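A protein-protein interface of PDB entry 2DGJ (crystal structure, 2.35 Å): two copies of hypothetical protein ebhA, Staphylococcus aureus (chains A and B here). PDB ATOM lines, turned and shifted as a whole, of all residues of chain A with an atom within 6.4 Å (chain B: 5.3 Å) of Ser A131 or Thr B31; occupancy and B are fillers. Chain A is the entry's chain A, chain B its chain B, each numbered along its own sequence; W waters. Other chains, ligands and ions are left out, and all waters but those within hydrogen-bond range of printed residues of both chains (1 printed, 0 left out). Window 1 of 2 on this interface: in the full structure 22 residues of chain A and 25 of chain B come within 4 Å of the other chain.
Ser A131 touches just one residue of chain B: Thr B31. Of the printed residues of chain A, Gln B35 touches Leu A187. Printed residues of chain B within 4 Å of Ala A128: Gln B27. Of the printed residues of chain A, Gln B27 touches Gly A127 (3.6 Å) and Ala A128 (3.4 Å). Printed residues of chain B within 4 Å of Leu A187: Gln B35 (3.3 Å). Gln A133 touches none of the printed residues of chain B. The nearest residue of chain A that does not touch Thr B31 is Leu A187 (4.9 Å).
Water W1 lies within hydrogen-bond range of the side-chain hydroxyl of Ser A131 (2.8 Å), the side-chain amide nitrogen of Gln B27 (3.2 Å) and the backbone carbonyl oxygen of Gly A127 (3.4 Å).
The side-chain amide nitrogen of Gln B27 lies close to the backbone NH of Ala A128 (3.4 Å).
Gln B27 touches Gly A127 (NE2 to C, 3.6 Å). Ser A131 touches Thr B31. Leu A187 touches Gln B35 (CG to OE1, 3.3 Å).
The backbone carbonyl oxygen (O) of Gly A127 is in hydrogen-bond range of the side-chain hydroxyl (OG) of Ser A131 (3.2 Å). O of Ser B28 lies within hydrogen-bond range of OG1 of Thr B31. OD2 of Asp B34 sits close to N of Thr B31, 3.4 Å away.
No position is printed for both chains. Of the 4 pairs that touch across the chains among the printed residues, none has its exchanged pair printed and touching as well.
Printed residues of chain A that touch a printed residue of chain B: Gly A127, Ala A128, Ser A131 and Leu A187. Of the 11 printed residues of chain B, 3 touch a printed residue of chain A. Printed residues of chain B that touch a printed residue of chain A: Gln B27, Thr B31 and Gln B35. Among the printed residues, no Asp or Glu carboxylate lies within 4 Å of a Lys or Arg side-chain nitrogen of the other chain.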
ATOM      1  N   ASP A 126      30.318   4.128  23.163  1.00  0.00           N
ATOM      2  CA  ASP A 126      31.032   4.436  24.397  1.00  0.00           C
ATOM      3  C   ASP A 126      30.154   5.308  25.290  1.00  0.00           C
ATOM      4  O   ASP A 126      30.136   5.148  26.509  1.00  0.00           O
ATOM      5  CB  ASP A 126      32.334   5.176  24.091  1.00  0.00           C
ATOM      6  CG  ASP A 126      33.191   5.382  25.326  1.00  0.00           C
ATOM      7  OD1 ASP A 126      33.742   4.384  25.840  1.00  0.00           O
ATOM      8  OD2 ASP A 126      33.306   6.534  25.792  1.00  0.00           O
ATOM      9  N   GLY A 127      29.435   6.242  24.674  1.00  0.00           N
ATOM     10  CA  GLY A 127      28.565   7.116  25.437  1.00  0.00           C
ATOM     11  C   GLY A 127      27.483   6.318  26.139  1.00  0.00           C
ATOM     12  O   GLY A 127      27.154   6.577  27.293  1.00  0.00           O
ATOM     13  N   ALA A 128      26.930   5.336  25.435  1.00  0.00           N
ATOM     14  CA  ALA A 128      25.880   4.489  25.989  1.00  0.00           C
ATOM     15  C   ALA A 128      26.433   3.613  27.109  1.00  0.00           C
ATOM     16  O   ALA A 128      25.794   3.445  28.150  1.00  0.00           O
ATOM     17  CB  ALA A 128      25.282   3.629  24.889  1.00  0.00           C
ATOM     18  N   MET A 129      27.619   3.052  26.891  1.00  0.00           N
ATOM     19  CA  MET A 129      28.263   2.216  27.896  1.00  0.00           C
ATOM     20  C   MET A 129      28.480   3.060  29.146  1.00  0.00           C
ATOM     21  O   MET A 129      28.275   2.595  30.265  1.00  0.00           O
ATOM     22  CB  MET A 129      29.611   1.704  27.388  1.00  0.00           C
ATOM     23  CG  MET A 129      29.518   0.620  26.329  1.00  0.00           C
ATOM     24  SD  MET A 129      28.819  -1.038  27.038  1.00  0.00           S
ATOM     25  CE  MET A 129      30.447  -1.749  27.801  1.00  0.00           C
ATOM     26  N   ASN A 130      28.886   4.308  28.942  1.00  0.00           N
ATOM     27  CA  ASN A 130      29.125   5.228  30.045  1.00  0.00           C
ATOM     28  C   ASN A 130      27.838   5.420  30.838  1.00  0.00           C
ATOM     29  O   ASN A 130      27.852   5.473  32.069  1.00  0.00           O
ATOM     30  CB  ASN A 130      29.604   6.574  29.500  1.00  0.00           C
ATOM     31  CG  ASN A 130      29.995   7.546  30.598  1.00  0.00           C
ATOM     32  OD1 ASN A 130      29.491   8.664  30.659  1.00  0.00           O
ATOM     33  ND2 ASN A 130      30.901   7.124  31.471  1.00  0.00           N
ATOM     34  N   SER A 131      26.725   5.524  30.122  1.00  0.00           N
ATOM     35  CA  SER A 131      25.430   5.713  30.755  1.00  0.00           C
ATOM     36  C   SER A 131      25.029   4.476  31.551  1.00  0.00           C
ATOM     37  O   SER A 131      24.550   4.579  32.683  1.00  0.00           O
ATOM     38  CB  SER A 131      24.366   6.017  29.701  1.00  0.00           C
ATOM     39  OG  SER A 131      24.614   7.252  29.048  1.00  0.00           O
ATOM     40  N   LEU A 132      25.236   3.304  30.959  1.00  0.00           N
ATOM     41  CA  LEU A 132      24.894   2.055  31.623  1.00  0.00           C
ATOM     42  C   LEU A 132      25.739   1.883  32.874  1.00  0.00           C
ATOM     43  O   LEU A 132      25.264   1.366  33.883  1.00  0.00           O
ATOM     44  CB  LEU A 132      25.119   0.867  30.687  1.00  0.00           C
ATOM     45  CG  LEU A 132      24.799  -0.521  31.252  1.00  0.00           C
ATOM     46  CD1 LEU A 132      23.380  -0.549  31.787  1.00  0.00           C
ATOM     47  CD2 LEU A 132      24.971  -1.569  30.164  1.00  0.00           C
ATOM     48  N   GLN A 133      26.989   2.325  32.802  1.00  0.00           N
ATOM     49  CA  GLN A 133      27.904   2.228  33.938  1.00  0.00           C
ATOM     50  C   GLN A 133      27.418   3.138  35.063  1.00  0.00           C
ATOM     51  O   GLN A 133      27.458   2.765  36.238  1.00  0.00           O
ATOM     52  CB  GLN A 133      29.319   2.650  33.518  1.00  0.00           C
ATOM     53  CG  GLN A 133      30.345   2.633  34.648  1.00  0.00           C
ATOM     54  CD  GLN A 133      30.563   1.244  35.217  1.00  0.00           C
ATOM     55  OE1 GLN A 133      30.999   0.333  34.513  1.00  0.00           O
ATOM     56  NE2 GLN A 133      30.257   1.073  36.498  1.00  0.00           N
ATOM     57  N   GLY A 134      26.962   4.333  34.700  1.00  0.00           N
ATOM     58  CA  GLY A 134      26.488   5.272  35.699  1.00  0.00           C
ATOM     59  C   GLY A 134      25.208   4.817  36.364  1.00  0.00           C
ATOM     60  O   GLY A 134      24.999   5.049  37.554  1.00  0.00           O
ATOM     61  N   ALA A 135      24.345   4.160  35.598  1.00  0.00           N
ATOM     62  CA  ALA A 135      23.076   3.675  36.115  1.00  0.00           C
ATOM     63  C   ALA A 135      23.250   2.663  37.247  1.00  0.00           C
ATOM     64  O   ALA A 135      22.355   2.499  38.073  1.00  0.00           O
ATOM     65  CB  ALA A 135      22.259   3.057  34.987  1.00  0.00           C
ATOM     66  N   ILE A 136      24.397   1.991  37.287  1.00  0.00           N
ATOM     67  CA  ILE A 136      24.631   0.996  38.329  1.00  0.00           C
ATOM     68  C   ILE A 136      25.797   1.316  39.267  1.00  0.00           C
ATOM     69  O   ILE A 136      26.295   0.429  39.957  1.00  0.00           O
ATOM     70  CB  ILE A 136      24.879  -0.411  37.725  1.00  0.00           C
ATOM     71  CG1 ILE A 136      26.252  -0.459  37.051  1.00  0.00           C
ATOM     72  CG2 ILE A 136      23.788  -0.746  36.713  1.00  0.00           C
ATOM     73  CD1 ILE A 136      26.675  -1.858  36.646  1.00  0.00           C
ATOM     74  N   ASP A 184      21.452   0.027  25.321  1.00  0.00           N
ATOM     75  CA  ASP A 184      20.316   0.861  25.687  1.00  0.00           C
ATOM     76  C   ASP A 184      19.221   0.029  26.340  1.00  0.00           C
ATOM     77  O   ASP A 184      18.547   0.493  27.258  1.00  0.00           O
ATOM     78  CB  ASP A 184      19.750   1.594  24.466  1.00  0.00           C
ATOM     79  CG  ASP A 184      20.637   2.748  24.019  1.00  0.00           C
ATOM     80  OD1 ASP A 184      21.325   3.337  24.878  1.00  0.00           O
ATOM     81  OD2 ASP A 184      20.633   3.079  22.811  1.00  0.00           O
ATOM     82  N   LEU A 187      20.368  -0.526  29.794  1.00  0.00           N
ATOM     83  CA  LEU A 187      20.250   0.709  30.560  1.00  0.00           C
ATOM     84  C   LEU A 187      18.822   0.909  31.056  1.00  0.00           C
ATOM     85  O   LEU A 187      18.595   1.149  32.245  1.00  0.00           O
ATOM     86  CB  LEU A 187      20.672   1.905  29.704  1.00  0.00           C
ATOM     87  CG  LEU A 187      20.367   3.301  30.255  1.00  0.00           C
ATOM     88  CD1 LEU A 187      20.918   3.428  31.656  1.00  0.00           C
ATOM     89  CD2 LEU A 187      20.975   4.356  29.345  1.00  0.00           C
ATOM     90  N   GLU B  26      23.480  17.104  23.418  1.00  0.00           N
ATOM     91  CA  GLU B  26      24.538  16.115  23.607  1.00  0.00           C
ATOM     92  C   GLU B  26      23.920  14.762  23.953  1.00  0.00           C
ATOM     93  O   GLU B  26      22.894  14.690  24.642  1.00  0.00           O
ATOM     94  CB  GLU B  26      25.487  16.564  24.721  1.00  0.00           C
ATOM     95  CG  GLU B  26      26.382  17.724  24.315  1.00  0.00           C
ATOM     96  CD  GLU B  26      27.121  18.337  25.488  1.00  0.00           C
ATOM     97  OE1 GLU B  26      27.741  17.583  26.266  1.00  0.00           O
ATOM     98  OE2 GLU B  26      27.080  19.580  25.627  1.00  0.00           O
ATOM     99  N   GLN B  27      24.546  13.691  23.475  1.00  0.00           N
ATOM    100  CA  GLN B  27      24.045  12.344  23.719  1.00  0.00           C
ATOM    101  C   GLN B  27      23.678  12.141  25.184  1.00  0.00           C
ATOM    102  O   GLN B  27      22.567  11.713  25.499  1.00  0.00           O
ATOM    103  CB  GLN B  27      25.087  11.304  23.301  1.00  0.00           C
ATOM    104  CG  GLN B  27      24.532   9.885  23.199  1.00  0.00           C
ATOM    105  CD  GLN B  27      25.584   8.879  22.776  1.00  0.00           C
ATOM    106  OE1 GLN B  27      26.414   9.164  21.913  1.00  0.00           O
ATOM    107  NE2 GLN B  27      25.548   7.690  23.371  1.00  0.00           N
ATOM    108  N   SER B  28      24.615  12.458  26.072  1.00  0.00           N
ATOM    109  CA  SER B  28      24.404  12.309  27.507  1.00  0.00           C
ATOM    110  C   SER B  28      23.157  13.053  27.973  1.00  0.00           C
ATOM    111  O   SER B  28      22.378  12.535  28.773  1.00  0.00           O
ATOM    112  CB  SER B  28      25.624  12.827  28.279  1.00  0.00           C
ATOM    113  OG  SER B  28      25.811  14.219  28.082  1.00  0.00           O
ATOM    114  N   LYS B  29      22.974  14.270  27.472  1.00  0.00           N
ATOM    115  CA  LYS B  29      21.825  15.085  27.851  1.00  0.00           C
ATOM    116  C   LYS B  29      20.524  14.422  27.401  1.00  0.00           C
ATOM    117  O   LYS B  29      19.524  14.439  28.117  1.00  0.00           O
ATOM    118  CB  LYS B  29      21.937  16.481  27.227  1.00  0.00           C
ATOM    119  CG  LYS B  29      23.170  17.289  27.653  1.00  0.00           C
ATOM    120  CD  LYS B  29      23.048  17.782  29.086  1.00  0.00           C
ATOM    121  CE  LYS B  29      24.190  18.721  29.466  1.00  0.00           C
ATOM    122  NZ  LYS B  29      25.516  18.047  29.494  1.00  0.00           N
ATOM    123  N   LYS B  30      20.549  13.830  26.212  1.00  0.00           N
ATOM    124  CA  LYS B  30      19.372  13.165  25.666  1.00  0.00           C
ATOM    125  C   LYS B  30      18.985  11.921  26.452  1.00  0.00           C
ATOM    126  O   LYS B  30      17.828  11.770  26.850  1.00  0.00           O
ATOM    127  CB  LYS B  30      19.612  12.796  24.197  1.00  0.00           C
ATOM    128  CG  LYS B  30      19.816  13.998  23.292  1.00  0.00           C
ATOM    129  CD  LYS B  30      20.188  13.610  21.858  1.00  0.00           C
ATOM    130  CE  LYS B  30      19.034  12.958  21.108  1.00  0.00           C
ATOM    131  NZ  LYS B  30      19.395  12.667  19.685  1.00  0.00           N
ATOM    132  N   THR B  31      19.949  11.033  26.685  1.00  0.00           N
ATOM    133  CA  THR B  31      19.683   9.804  27.421  1.00  0.00           C
ATOM    134  C   THR B  31      19.240  10.117  28.850  1.00  0.00           C
ATOM    135  O   THR B  31      18.342   9.468  29.390  1.00  0.00           O
ATOM    136  CB  THR B  31      20.934   8.900  27.483  1.00  0.00           C
ATOM    137  OG1 THR B  31      21.917   9.500  28.332  1.00  0.00           O
ATOM    138  CG2 THR B  31      21.536   8.728  26.104  1.00  0.00           C
ATOM    139  N   ALA B  32      19.884  11.111  29.455  1.00  0.00           N
ATOM    140  CA  ALA B  32      19.553  11.511  30.816  1.00  0.00           C
ATOM    141  C   ALA B  32      18.071  11.869  30.877  1.00  0.00           C
ATOM    142  O   ALA B  32      17.395  11.597  31.866  1.00  0.00           O
ATOM    143  CB  ALA B  32      20.402  12.705  31.230  1.00  0.00           C
ATOM    144  N   TYR B  33      17.571  12.472  29.803  1.00  0.00           N
ATOM    145  CA  TYR B  33      16.166  12.856  29.732  1.00  0.00           C
ATOM    146  C   TYR B  33      15.265  11.642  29.529  1.00  0.00           C
ATOM    147  O   TYR B  33      14.258  11.481  30.227  1.00  0.00           O
ATOM    148  CB  TYR B  33      15.939  13.851  28.589  1.00  0.00           C
ATOM    149  CG  TYR B  33      14.480  14.173  28.366  1.00  0.00           C
ATOM    150  CD1 TYR B  33      13.728  14.788  29.364  1.00  0.00           C
ATOM    151  CD2 TYR B  33      13.844  13.829  27.176  1.00  0.00           C
ATOM    152  CE1 TYR B  33      12.373  15.049  29.186  1.00  0.00           C
ATOM    153  CE2 TYR B  33      12.489  14.084  26.985  1.00  0.00           C
ATOM    154  CZ  TYR B  33      11.760  14.694  27.997  1.00  0.00           C
ATOM    155  OH  TYR B  33      10.422  14.949  27.823  1.00  0.00           O
ATOM    156  N   ASP B  34      15.624  10.789  28.572  1.00  0.00           N
ATOM    157  CA  ASP B  34      14.822   9.606  28.280  1.00  0.00           C
ATOM    158  C   ASP B  34      14.677   8.744  29.525  1.00  0.00           C
ATOM    159  O   ASP B  34      13.584   8.298  29.867  1.00  0.00           O
ATOM    160  CB  ASP B  34      15.469   8.779  27.168  1.00  0.00           C
ATOM    161  CG  ASP B  34      16.036   9.639  26.054  1.00  0.00           C
ATOM    162  OD1 ASP B  34      15.351  10.585  25.608  1.00  0.00           O
ATOM    163  OD2 ASP B  34      17.175   9.363  25.618  1.00  0.00           O
ATOM    164  N   GLN B  35      15.793   8.522  30.205  1.00  0.00           N
ATOM    165  CA  GLN B  35      15.807   7.707  31.411  1.00  0.00           C
ATOM    166  C   GLN B  35      15.016   8.340  32.547  1.00  0.00           C
ATOM    167  O   GLN B  35      14.442   7.635  33.371  1.00  0.00           O
ATOM    168  CB  GLN B  35      17.248   7.452  31.852  1.00  0.00           C
ATOM    169  CG  GLN B  35      18.055   6.709  30.807  1.00  0.00           C
ATOM    170  CD  GLN B  35      17.395   5.408  30.389  1.00  0.00           C
ATOM    171  OE1 GLN B  35      17.420   4.421  31.125  1.00  0.00           O
ATOM    172  NE2 GLN B  35      16.793   5.408  29.204  1.00  0.00           N
ATOM    173  N   ALA B  36      14.994   9.667  32.590  1.00  0.00           N
ATOM    174  CA  ALA B  36      14.249  10.382  33.621  1.00  0.00           C
ATOM    175  C   ALA B  36      12.768  10.074  33.430  1.00  0.00           C
ATOM    176  O   ALA B  36      12.019   9.929  34.397  1.00  0.00           O
ATOM    177  CB  ALA B  36      14.496  11.890  33.510  1.00  0.00           C
HETATM  178  O   HOH W   1      24.101   7.494  26.256  1.00  0.00           O
